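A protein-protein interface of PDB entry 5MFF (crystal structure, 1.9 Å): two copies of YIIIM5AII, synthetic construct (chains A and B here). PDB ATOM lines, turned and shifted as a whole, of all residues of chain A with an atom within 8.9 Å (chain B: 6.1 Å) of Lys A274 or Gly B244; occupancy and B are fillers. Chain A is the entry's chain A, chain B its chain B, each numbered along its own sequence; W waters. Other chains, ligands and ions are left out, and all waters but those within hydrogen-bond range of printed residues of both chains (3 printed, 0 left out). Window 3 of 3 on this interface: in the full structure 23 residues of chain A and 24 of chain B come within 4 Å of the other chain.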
ATOM      1  N   GLN A 232      25.494   4.535  17.406  1.00  0.00           N
ATOM      2  CA  GLN A 232      24.616   5.221  16.460  1.00  0.00           C
ATOM      3  C   GLN A 232      25.282   5.386  15.073  1.00  0.00           C
ATOM      4  O   GLN A 232      24.639   5.135  14.056  1.00  0.00           O
ATOM      5  CB  GLN A 232      24.186   6.588  17.025  1.00  0.00           C
ATOM      6  CG  GLN A 232      23.478   7.490  16.023  1.00  0.00           C
ATOM      7  CD  GLN A 232      22.857   8.689  16.703  1.00  0.00           C
ATOM      8  OE1 GLN A 232      23.530   9.681  17.041  1.00  0.00           O
ATOM      9  NE2 GLN A 232      21.562   8.602  16.951  1.00  0.00           N
ATOM     10  N   LEU A 235      25.521   1.994  13.396  1.00  0.00           N
ATOM     11  CA  LEU A 235      24.147   1.660  12.981  1.00  0.00           C
ATOM     12  C   LEU A 235      23.747   2.374  11.688  1.00  0.00           C
ATOM     13  O   LEU A 235      23.125   1.755  10.814  1.00  0.00           O
ATOM     14  CB  LEU A 235      23.131   2.005  14.081  1.00  0.00           C
ATOM     15  CG  LEU A 235      22.722   0.873  14.982  1.00  0.00           C
ATOM     16  CD1 LEU A 235      21.870   1.385  16.132  1.00  0.00           C
ATOM     17  CD2 LEU A 235      21.995  -0.199  14.202  1.00  0.00           C
ATOM     18  N   TRP A 236      24.073   3.686  11.576  1.00  0.00           N
ATOM     19  CA  TRP A 236      23.784   4.487  10.383  1.00  0.00           C
ATOM     20  C   TRP A 236      24.606   3.992   9.183  1.00  0.00           C
ATOM     21  O   TRP A 236      24.049   3.879   8.096  1.00  0.00           O
ATOM     22  CB  TRP A 236      23.949   6.008  10.640  1.00  0.00           C
ATOM     23  CG  TRP A 236      23.550   6.881   9.479  1.00  0.00           C
ATOM     24  CD1 TRP A 236      24.362   7.717   8.769  1.00  0.00           C
ATOM     25  CD2 TRP A 236      22.244   6.985   8.878  1.00  0.00           C
ATOM     26  NE1 TRP A 236      23.659   8.298   7.736  1.00  0.00           N
ATOM     27  CE2 TRP A 236      22.358   7.859   7.776  1.00  0.00           C
ATOM     28  CE3 TRP A 236      20.996   6.399   9.145  1.00  0.00           C
ATOM     29  CZ2 TRP A 236      21.264   8.190   6.966  1.00  0.00           C
ATOM     30  CZ3 TRP A 236      19.917   6.719   8.341  1.00  0.00           C
ATOM     31  CH2 TRP A 236      20.054   7.601   7.263  1.00  0.00           C
ATOM     32  N   SER A 239      22.972   0.631   8.202  1.00  0.00           N
ATOM     33  CA  SER A 239      21.667   0.951   7.601  1.00  0.00           C
ATOM     34  C   SER A 239      21.830   1.485   6.166  1.00  0.00           C
ATOM     35  O   SER A 239      21.018   1.147   5.301  1.00  0.00           O
ATOM     36  CB  SER A 239      20.923   1.981   8.438  1.00  0.00           C
ATOM     37  OG  SER A 239      19.547   1.937   8.109  1.00  0.00           O
ATOM     38  N   LEU A 261      21.473  -6.738  15.555  1.00  0.00           N
ATOM     39  CA  LEU A 261      20.446  -5.769  15.136  1.00  0.00           C
ATOM     40  C   LEU A 261      19.102  -6.025  15.847  1.00  0.00           C
ATOM     41  O   LEU A 261      18.493  -5.083  16.354  1.00  0.00           O
ATOM     42  CB  LEU A 261      20.288  -5.698  13.603  1.00  0.00           C
ATOM     43  CG  LEU A 261      21.437  -5.031  12.823  1.00  0.00           C
ATOM     44  CD1 LEU A 261      21.190  -5.111  11.317  1.00  0.00           C
ATOM     45  CD2 LEU A 261      21.667  -3.572  13.263  1.00  0.00           C
ATOM     46  N   LEU A 264      19.445  -5.073  19.560  1.00  0.00           N
ATOM     47  CA  LEU A 264      19.461  -3.614  19.736  1.00  0.00           C
ATOM     48  C   LEU A 264      18.067  -2.970  19.641  1.00  0.00           C
ATOM     49  O   LEU A 264      17.899  -1.845  20.096  1.00  0.00           O
ATOM     50  CB  LEU A 264      20.469  -2.915  18.808  1.00  0.00           C
ATOM     51  CG  LEU A 264      21.967  -3.158  19.104  1.00  0.00           C
ATOM     52  CD1 LEU A 264      22.817  -2.713  17.939  1.00  0.00           C
ATOM     53  CD2 LEU A 264      22.410  -2.445  20.366  1.00  0.00           C
ATOM     54  N   GLN A 265      17.055  -3.711  19.151  1.00  0.00           N
ATOM     55  CA  GLN A 265      15.662  -3.236  19.139  1.00  0.00           C
ATOM     56  C   GLN A 265      15.166  -3.090  20.603  1.00  0.00           C
ATOM     57  O   GLN A 265      14.167  -2.412  20.840  1.00  0.00           O
ATOM     58  CB  GLN A 265      14.742  -4.188  18.339  1.00  0.00           C
ATOM     59  CG  GLN A 265      15.002  -4.149  16.827  1.00  0.00           C
ATOM     60  CD  GLN A 265      14.182  -5.162  16.057  1.00  0.00           C
ATOM     61  OE1 GLN A 265      14.076  -6.343  16.420  1.00  0.00           O
ATOM     62  NE2 GLN A 265      13.628  -4.737  14.942  1.00  0.00           N
ATOM     63  N   SER A 266      15.867  -3.722  21.574  1.00  0.00           N
ATOM     64  CA  SER A 266      15.525  -3.639  22.996  1.00  0.00           C
ATOM     65  C   SER A 266      16.545  -2.850  23.812  1.00  0.00           C
ATOM     66  O   SER A 266      16.511  -2.922  25.044  1.00  0.00           O
ATOM     67  CB  SER A 266      15.335  -5.032  23.591  1.00  0.00           C
ATOM     68  OG  SER A 266      14.292  -5.717  22.924  1.00  0.00           O
ATOM     69  N   HIS A 267      17.468  -2.104  23.140  1.00  0.00           N
ATOM     70  CA  HIS A 267      18.495  -1.282  23.815  1.00  0.00           C
ATOM     71  C   HIS A 267      17.789  -0.218  24.670  1.00  0.00           C
ATOM     72  O   HIS A 267      16.702   0.204  24.304  1.00  0.00           O
ATOM     73  CB  HIS A 267      19.379  -0.604  22.754  1.00  0.00           C
ATOM     74  CG  HIS A 267      20.556   0.145  23.294  1.00  0.00           C
ATOM     75  ND1 HIS A 267      20.424   1.423  23.812  1.00  0.00           N
ATOM     76  CD2 HIS A 267      21.861  -0.211  23.332  1.00  0.00           C
ATOM     77  CE1 HIS A 267      21.637   1.781  24.184  1.00  0.00           C
ATOM     78  NE2 HIS A 267      22.537   0.833  23.899  1.00  0.00           N
ATOM     79  N   ASN A 269      18.321   3.001  24.978  1.00  0.00           N
ATOM     80  CA  ASN A 269      18.098   4.210  24.187  1.00  0.00           C
ATOM     81  C   ASN A 269      17.066   3.958  23.080  1.00  0.00           C
ATOM     82  O   ASN A 269      17.313   3.188  22.153  1.00  0.00           O
ATOM     83  CB  ASN A 269      19.412   4.728  23.627  1.00  0.00           C
ATOM     84  CG  ASN A 269      19.321   6.100  23.009  1.00  0.00           C
ATOM     85  OD1 ASN A 269      18.468   6.392  22.158  1.00  0.00           O
ATOM     86  ND2 ASN A 269      20.256   6.943  23.359  1.00  0.00           N
ATOM     87  N   GLU A 270      15.920   4.635  23.182  1.00  0.00           N
ATOM     88  CA  GLU A 270      14.820   4.512  22.229  1.00  0.00           C
ATOM     89  C   GLU A 270      15.194   4.903  20.803  1.00  0.00           C
ATOM     90  O   GLU A 270      14.604   4.372  19.869  1.00  0.00           O
ATOM     91  CB  GLU A 270      13.588   5.266  22.707  1.00  0.00           C
ATOM     92  CG  GLU A 270      12.862   4.492  23.792  1.00  0.00           C
ATOM     93  CD  GLU A 270      11.824   5.310  24.526  1.00  0.00           C
ATOM     94  OE1 GLU A 270      11.877   5.351  25.778  1.00  0.00           O
ATOM     95  OE2 GLU A 270      10.974   5.932  23.848  1.00  0.00           O
ATOM     96  N   LYS A 271      16.171   5.796  20.623  1.00  0.00           N
ATOM     97  CA  LYS A 271      16.602   6.124  19.276  1.00  0.00           C
ATOM     98  C   LYS A 271      17.402   4.973  18.659  1.00  0.00           C
ATOM     99  O   LYS A 271      17.195   4.673  17.487  1.00  0.00           O
ATOM    100  CB  LYS A 271      17.329   7.468  19.183  1.00  0.00           C
ATOM    101  CG  LYS A 271      17.700   7.852  17.755  1.00  0.00           C
ATOM    102  CD  LYS A 271      16.490   7.973  16.811  1.00  0.00           C
ATOM    103  CE  LYS A 271      16.817   8.871  15.642  1.00  0.00           C
ATOM    104  NZ  LYS A 271      15.581   9.299  14.948  1.00  0.00           N
ATOM    105  N   ILE A 272      18.256   4.296  19.461  1.00  0.00           N
ATOM    106  CA  ILE A 272      19.002   3.103  19.033  1.00  0.00           C
ATOM    107  C   ILE A 272      18.001   2.033  18.564  1.00  0.00           C
ATOM    108  O   ILE A 272      18.196   1.432  17.501  1.00  0.00           O
ATOM    109  CB  ILE A 272      19.972   2.559  20.146  1.00  0.00           C
ATOM    110  CG1 ILE A 272      21.079   3.605  20.549  1.00  0.00           C
ATOM    111  CG2 ILE A 272      20.581   1.197  19.755  1.00  0.00           C
ATOM    112  CD1 ILE A 272      22.064   4.130  19.464  1.00  0.00           C
ATOM    113  N   GLN A 273      16.927   1.819  19.356  1.00  0.00           N
ATOM    114  CA  GLN A 273      15.862   0.864  19.058  1.00  0.00           C
ATOM    115  C   GLN A 273      15.317   1.104  17.628  1.00  0.00           C
ATOM    116  O   GLN A 273      15.300   0.172  16.819  1.00  0.00           O
ATOM    117  CB  GLN A 273      14.723   0.989  20.077  1.00  0.00           C
ATOM    118  CG  GLN A 273      15.086   0.605  21.513  1.00  0.00           C
ATOM    119  CD  GLN A 273      13.861   0.546  22.413  1.00  0.00           C
ATOM    120  OE1 GLN A 273      12.711   0.722  21.979  1.00  0.00           O
ATOM    121  NE2 GLN A 273      14.071   0.281  23.693  1.00  0.00           N
ATOM    122  N   LYS A 274      14.922   2.366  17.325  1.00  0.00           N
ATOM    123  CA  LYS A 274      14.369   2.793  16.029  1.00  0.00           C
ATOM    124  C   LYS A 274      15.351   2.561  14.879  1.00  0.00           C
ATOM    125  O   LYS A 274      14.958   2.020  13.845  1.00  0.00           O
ATOM    126  CB  LYS A 274      13.963   4.281  16.063  1.00  0.00           C
ATOM    127  CG  LYS A 274      12.775   4.566  16.966  1.00  0.00           C
ATOM    128  CD  LYS A 274      12.535   6.067  17.047  1.00  0.00           C
ATOM    129  CE  LYS A 274      11.220   6.395  17.698  1.00  0.00           C
ATOM    130  NZ  LYS A 274      10.060   5.867  16.917  1.00  0.00           N
ATOM    131  N   GLU A 275      16.623   2.963  15.068  1.00  0.00           N
ATOM    132  CA  GLU A 275      17.700   2.806  14.074  1.00  0.00           C
ATOM    133  C   GLU A 275      17.973   1.310  13.816  1.00  0.00           C
ATOM    134  O   GLU A 275      18.129   0.926  12.660  1.00  0.00           O
ATOM    135  CB  GLU A 275      18.992   3.515  14.522  1.00  0.00           C
ATOM    136  CG  GLU A 275      18.781   4.974  14.907  1.00  0.00           C
ATOM    137  CD  GLU A 275      19.921   5.723  15.576  1.00  0.00           C
ATOM    138  OE1 GLU A 275      20.854   5.077  16.103  1.00  0.00           O
ATOM    139  OE2 GLU A 275      19.878   6.973  15.565  1.00  0.00           O
ATOM    140  N   ALA A 276      18.004   0.472  14.879  1.00  0.00           N
ATOM    141  CA  ALA A 276      18.205  -0.978  14.736  1.00  0.00           C
ATOM    142  C   ALA A 276      17.007  -1.591  14.001  1.00  0.00           C
ATOM    143  O   ALA A 276      17.201  -2.405  13.098  1.00  0.00           O
ATOM    144  CB  ALA A 276      18.378  -1.637  16.101  1.00  0.00           C
ATOM    145  N   GLN A 277      15.771  -1.168  14.359  1.00  0.00           N
ATOM    146  CA  GLN A 277      14.556  -1.652  13.704  1.00  0.00           C
ATOM    147  C   GLN A 277      14.553  -1.291  12.210  1.00  0.00           C
ATOM    148  O   GLN A 277      14.293  -2.160  11.383  1.00  0.00           O
ATOM    149  CB  GLN A 277      13.297  -1.114  14.402  1.00  0.00           C
ATOM    150  CG  GLN A 277      12.003  -1.744  13.887  1.00  0.00           C
ATOM    151  CD  GLN A 277      10.820  -1.411  14.757  1.00  0.00           C
ATOM    152  OE1 GLN A 277      10.512  -0.242  15.023  1.00  0.00           O
ATOM    153  NE2 GLN A 277      10.118  -2.439  15.206  1.00  0.00           N
ATOM    154  N   GLU A 278      14.881  -0.041  11.875  1.00  0.00           N
ATOM    155  CA  GLU A 278      14.950   0.440  10.494  1.00  0.00           C
ATOM    156  C   GLU A 278      15.988  -0.371   9.684  1.00  0.00           C
ATOM    157  O   GLU A 278      15.684  -0.789   8.560  1.00  0.00           O
ATOM    158  CB  GLU A 278      15.285   1.944  10.481  1.00  0.00           C
ATOM    159  CG  GLU A 278      15.229   2.605   9.118  1.00  0.00           C
ATOM    160  CD  GLU A 278      15.673   4.051   9.150  1.00  0.00           C
ATOM    161  OE1 GLU A 278      16.889   4.303   8.992  1.00  0.00           O
ATOM    162  OE2 GLU A 278      14.808   4.933   9.359  1.00  0.00           O
ATOM    163  N   ALA A 279      17.193  -0.614  10.278  1.00  0.00           N
ATOM    164  CA  ALA A 279      18.281  -1.381   9.657  1.00  0.00           C
ATOM    165  C   ALA A 279      17.838  -2.815   9.364  1.00  0.00           C
ATOM    166  O   ALA A 279      17.971  -3.283   8.227  1.00  0.00           O
ATOM    167  CB  ALA A 279      19.511  -1.388  10.556  1.00  0.00           C
ATOM    168  N   LEU A 280      17.272  -3.484  10.379  1.00  0.00           N
ATOM    169  CA  LEU A 280      16.793  -4.862  10.287  1.00  0.00           C
ATOM    170  C   LEU A 280      15.651  -5.015   9.268  1.00  0.00           C
ATOM    171  O   LEU A 280      15.616  -6.011   8.550  1.00  0.00           O
ATOM    172  CB  LEU A 280      16.400  -5.378  11.689  1.00  0.00           C
ATOM    173  CG  LEU A 280      16.169  -6.876  11.849  1.00  0.00           C
ATOM    174  CD1 LEU A 280      17.487  -7.647  11.921  1.00  0.00           C
ATOM    175  CD2 LEU A 280      15.369  -7.148  13.092  1.00  0.00           C
ATOM    176  N   GLU A 281      14.772  -4.007   9.163  1.00  0.00           N
ATOM    177  CA  GLU A 281      13.654  -3.996   8.218  1.00  0.00           C
ATOM    178  C   GLU A 281      14.127  -3.886   6.769  1.00  0.00           C
ATOM    179  O   GLU A 281      13.551  -4.540   5.899  1.00  0.00           O
ATOM    180  CB  GLU A 281      12.635  -2.900   8.565  1.00  0.00           C
ATOM    181  CG  GLU A 281      11.673  -3.336   9.669  1.00  0.00           C
ATOM    182  CD  GLU A 281      10.762  -2.287  10.287  1.00  0.00           C
ATOM    183  OE1 GLU A 281      10.854  -1.097   9.905  1.00  0.00           O
ATOM    184  OE2 GLU A 281       9.958  -2.662  11.171  1.00  0.00           O
ATOM    185  N   LYS A 282      15.206  -3.109   6.523  1.00  0.00           N
ATOM    186  CA  LYS A 282      15.826  -2.958   5.202  1.00  0.00           C
ATOM    187  C   LYS A 282      16.400  -4.293   4.735  1.00  0.00           C
ATOM    188  O   LYS A 282      16.306  -4.615   3.552  1.00  0.00           O
ATOM    189  CB  LYS A 282      16.945  -1.911   5.228  1.00  0.00           C
ATOM    190  CG  LYS A 282      16.452  -0.487   5.185  1.00  0.00           C
ATOM    191  CD  LYS A 282      17.583   0.496   5.391  1.00  0.00           C
ATOM    192  CE  LYS A 282      17.029   1.830   5.817  1.00  0.00           C
ATOM    193  NZ  LYS A 282      17.739   2.962   5.176  1.00  0.00           N
ATOM    194  N   GLY B 202      14.987  11.867  19.634  1.00  0.00           N
ATOM    195  CA  GLY B 202      14.751  10.948  20.743  1.00  0.00           C
ATOM    196  C   GLY B 202      13.632   9.959  20.488  1.00  0.00           C
ATOM    197  O   GLY B 202      13.284   9.689  19.333  1.00  0.00           O
ATOM    198  N   GLY B 203      13.062   9.418  21.566  1.00  0.00           N
ATOM    199  CA  GLY B 203      11.936   8.491  21.473  1.00  0.00           C
ATOM    200  C   GLY B 203      10.626   9.195  21.133  1.00  0.00           C
ATOM    201  O   GLY B 203      10.590  10.434  20.979  1.00  0.00           O
ATOM    202  N   ASN B 204       9.532   8.402  21.017  1.00  0.00           N
ATOM    203  CA  ASN B 204       8.189   8.882  20.662  1.00  0.00           C
ATOM    204  C   ASN B 204       7.656   9.964  21.586  1.00  0.00           C
ATOM    205  O   ASN B 204       7.072  10.928  21.092  1.00  0.00           O
ATOM    206  CB  ASN B 204       7.186   7.731  20.530  1.00  0.00           C
ATOM    207  CG  ASN B 204       7.382   6.912  19.281  1.00  0.00           C
ATOM    208  OD1 ASN B 204       8.193   7.234  18.414  1.00  0.00           O
ATOM    209  ND2 ASN B 204       6.672   5.810  19.181  1.00  0.00           N
ATOM    210  N   ILE B 207       9.539  13.240  20.810  1.00  0.00           N
ATOM    211  CA  ILE B 207       9.017  13.762  19.548  1.00  0.00           C
ATOM    212  C   ILE B 207       7.633  14.367  19.815  1.00  0.00           C
ATOM    213  O   ILE B 207       7.331  15.463  19.315  1.00  0.00           O
ATOM    214  CB  ILE B 207       8.931  12.655  18.456  1.00  0.00           C
ATOM    215  CG1 ILE B 207      10.327  12.120  18.073  1.00  0.00           C
ATOM    216  CG2 ILE B 207       8.150  13.153  17.220  1.00  0.00           C
ATOM    217  CD1 ILE B 207      10.298  10.762  17.328  1.00  0.00           C
ATOM    218  N   SER B 239      12.256  15.345   9.486  1.00  0.00           N
ATOM    219  CA  SER B 239      12.662  13.966   9.203  1.00  0.00           C
ATOM    220  C   SER B 239      12.801  13.182  10.525  1.00  0.00           C
ATOM    221  O   SER B 239      12.311  12.048  10.613  1.00  0.00           O
ATOM    222  CB  SER B 239      13.966  13.937   8.406  1.00  0.00           C
ATOM    223  OG  SER B 239      14.346  12.609   8.088  1.00  0.00           O
ATOM    224  N   ASN B 240      13.388  13.825  11.572  1.00  0.00           N
ATOM    225  CA  ASN B 240      13.513  13.239  12.908  1.00  0.00           C
ATOM    226  C   ASN B 240      12.157  13.025  13.542  1.00  0.00           C
ATOM    227  O   ASN B 240      11.925  11.961  14.126  1.00  0.00           O
ATOM    228  CB  ASN B 240      14.415  14.067  13.821  1.00  0.00           C
ATOM    229  CG  ASN B 240      15.877  13.714  13.715  1.00  0.00           C
ATOM    230  OD1 ASN B 240      16.732  14.585  13.616  1.00  0.00           O
ATOM    231  ND2 ASN B 240      16.203  12.433  13.802  1.00  0.00           N
ATOM    232  N   ILE B 241      11.237  13.991  13.377  1.00  0.00           N
ATOM    233  CA  ILE B 241       9.858  13.876  13.882  1.00  0.00           C
ATOM    234  C   ILE B 241       9.133  12.686  13.206  1.00  0.00           C
ATOM    235  O   ILE B 241       8.459  11.895  13.894  1.00  0.00           O
ATOM    236  CB  ILE B 241       9.073  15.222  13.779  1.00  0.00           C
ATOM    237  CG1 ILE B 241       9.717  16.282  14.702  1.00  0.00           C
ATOM    238  CG2 ILE B 241       7.585  15.025  14.134  1.00  0.00           C
ATOM    239  CD1 ILE B 241       9.149  17.688  14.623  1.00  0.00           C
ATOM    240  N   ALA B 242       9.313  12.553  11.866  1.00  0.00           N
ATOM    241  CA  ALA B 242       8.742  11.475  11.046  1.00  0.00           C
ATOM    242  C   ALA B 242       9.229  10.072  11.491  1.00  0.00           C
ATOM    243  O   ALA B 242       8.597   9.080  11.138  1.00  0.00           O
ATOM    244  CB  ALA B 242       9.062  11.709   9.578  1.00  0.00           C
ATOM    245  N   SER B 243      10.316   9.997  12.292  1.00  0.00           N
ATOM    246  CA  SER B 243      10.849   8.749  12.874  1.00  0.00           C
ATOM    247  C   SER B 243       9.921   8.214  13.970  1.00  0.00           C
ATOM    248  O   SER B 243      10.077   7.070  14.384  1.00  0.00           O
ATOM    249  CB  SER B 243      12.252   8.950  13.451  1.00  0.00           C
ATOM    250  OG  SER B 243      13.205   9.102  12.415  1.00  0.00           O
ATOM    251  N   GLY B 244       8.962   9.030  14.415  1.00  0.00           N
ATOM    252  CA  GLY B 244       8.000   8.643  15.445  1.00  0.00           C
ATOM    253  C   GLY B 244       6.989   7.598  15.019  1.00  0.00           C
ATOM    254  O   GLY B 244       6.993   7.140  13.874  1.00  0.00           O
ATOM    255  N   GLY B 245       6.110   7.231  15.950  1.00  0.00           N
ATOM    256  CA  GLY B 245       5.024   6.286  15.719  1.00  0.00           C
ATOM    257  C   GLY B 245       3.917   6.919  14.891  1.00  0.00           C
ATOM    258  O   GLY B 245       4.044   8.074  14.473  1.00  0.00           O
ATOM    259  N   ASN B 246       2.816   6.178  14.658  1.00  0.00           N
ATOM    260  CA  ASN B 246       1.685   6.645  13.848  1.00  0.00           C
ATOM    261  C   ASN B 246       1.074   7.964  14.340  1.00  0.00           C
ATOM    262  O   ASN B 246       0.811   8.820  13.500  1.00  0.00           O
ATOM    263  CB  ASN B 246       0.606   5.568  13.674  1.00  0.00           C
ATOM    264  CG  ASN B 246       0.976   4.414  12.757  1.00  0.00           C
ATOM    265  OD1 ASN B 246       0.386   3.331  12.836  1.00  0.00           O
ATOM    266  ND2 ASN B 246       1.943   4.602  11.860  1.00  0.00           N
ATOM    267  N   GLN B 248       2.605  10.456  15.848  1.00  0.00           N
ATOM    268  CA  GLN B 248       3.558  11.490  15.458  1.00  0.00           C
ATOM    269  C   GLN B 248       3.501  11.718  13.933  1.00  0.00           C
ATOM    270  O   GLN B 248       3.397  12.868  13.492  1.00  0.00           O
ATOM    271  CB  GLN B 248       4.982  11.142  15.953  1.00  0.00           C
ATOM    272  CG  GLN B 248       5.156  11.249  17.482  1.00  0.00           C
ATOM    273  CD  GLN B 248       4.610  10.067  18.244  1.00  0.00           C
ATOM    274  OE1 GLN B 248       4.963   8.911  17.990  1.00  0.00           O
ATOM    275  NE2 GLN B 248       3.746  10.332  19.206  1.00  0.00           N
ATOM    276  N   LYS B 249       3.480  10.624  13.138  1.00  0.00           N
ATOM    277  CA  LYS B 249       3.401  10.701  11.673  1.00  0.00           C
ATOM    278  C   LYS B 249       2.107  11.414  11.216  1.00  0.00           C
ATOM    279  O   LYS B 249       2.153  12.249  10.309  1.00  0.00           O
ATOM    280  CB  LYS B 249       3.490   9.309  11.027  1.00  0.00           C
ATOM    281  CG  LYS B 249       4.830   8.586  11.188  1.00  0.00           C
ATOM    282  CD  LYS B 249       4.754   7.231  10.478  1.00  0.00           C
ATOM    283  CE  LYS B 249       5.685   6.177  11.019  1.00  0.00           C
ATOM    284  NZ  LYS B 249       7.111   6.509  10.781  1.00  0.00           N
ATOM    285  N   LYS B 282       9.682   7.796   5.533  1.00  0.00           N
ATOM    286  CA  LYS B 282       9.366   7.576   6.953  1.00  0.00           C
ATOM    287  C   LYS B 282       7.869   7.785   7.247  1.00  0.00           C
ATOM    288  O   LYS B 282       7.282   7.024   8.019  1.00  0.00           O
ATOM    289  CB  LYS B 282      10.182   8.519   7.845  1.00  0.00           C
ATOM    290  CG  LYS B 282      11.668   8.239   7.909  1.00  0.00           C
ATOM    291  CD  LYS B 282      12.315   9.163   8.919  1.00  0.00           C
ATOM    292  CE  LYS B 282      13.816   9.070   8.907  1.00  0.00           C
ATOM    293  NZ  LYS B 282      14.432  10.134   9.742  1.00  0.00           N
HETATM  294  O   HOH W   1       8.940   7.559  24.317  1.00  0.00           O
HETATM  295  O   HOH W   2       9.984   5.649  21.315  1.00  0.00           O
HETATM  296  O   HOH W   3      13.640  10.374  16.597  1.00  0.00           O
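Water W1 bridges the side-chain carboxylate of Glu A270 (2.6 Å) and the backbone NH of Asn B204 (3.5 Å). Water W2 lies within hydrogen-bond range of OE2 of Glu A270 (2.7 Å) and N of Asn B204 (2.8 Å). Water W3 lies within hydrogen-bond range of the side-chain amino group (NZ) of Lys A271 (2.8 Å), the backbone carbonyl oxygen (O) of Gly B202 (2.8 Å) and the backbone carbonyl oxygen (O) of Asn B240 (3.4 Å).
Gly B203 touches Glu A270. Lys A274 touches Gly B244 (NZ to CA, 3.8 Å).
The side-chain amino group (NZ) of Lys A271 lies close to the side-chain amide nitrogen (ND2) of Asn B240, 3.4 Å away. NZ of Lys A274 sits at hydrogen-bond distance from O of Ser B243, at 2.8 Å. NZ of Lys A271 is in hydrogen-bond range of OG of Ser B243 (3.5 Å). The side-chain amino group (NZ) of Lys A274 sits at hydrogen-bond distance from the side-chain amide oxygen (OD1) of Asn B204 (2.8 Å).
Printed residues of chain A that touch a printed residue of chain B: Glu A270, Lys A271 and Lys A274. Along chain A the printed residues that touch a printed residue of chain B span positions 270 to 274. Of the 15 printed residues of chain B, 5 touch a printed residue of chain A. Among the printed residues, 6 pairs touch across the chains. Among the printed residues, no Asp or Glu carboxylate lies within 4 Å of a Lys or Arg side-chain nitrogen of the other chain.
The backbone NH (N) of Gly B245 lies within hydrogen-bond range of the side-chain amide oxygen (OD1) of Asn B204 (3.2 Å). The backbone carbonyl oxygen of Gly B244 sits at hydrogen-bond distance from the side-chain amino group of Lys B249 (3.2 Å). The backbone NH (N) of Lys A271 sits at hydrogen-bond distance from the side-chain amide oxygen (OD1) of Asn A269 (2.8 Å). The side-chain hydroxyl (OG) of Ser B243 lies within hydrogen-bond range of the side-chain amino group (NZ) of Lys B282 (3.1 Å).
Positions printed for both chains: 239 and 282. Of the 6 pairs that touch across the chains among the printed residues, none has its exchanged pair printed and touching as well.
Leu A261 touches none of the printed residues of chain B. Of the printed residues of chain B, Lys A271 touches Asn B240 and Ser B243. Lys A274 touches just these residues of chain B: Asn B204, Ser B243 and Gly B244. Of the printed residues of chain A, Gly B203 touches Glu A270 (3.6 Å). Ser B243 touches just these residues of chain A: Lys A271 (3.5 Å) and Lys A274 (2.8 Å). Gly B244 touches just one residue of chain A: Lys A274. No residue of chain A comes within 4 Å of Gly B245. The nearest residue of chain B that does not touch Lys A274 is Gly B202 (4.2 Å). The nearest printed residue of chain A that does not touch Asn B204 is Glu A270 (4.02 Å).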
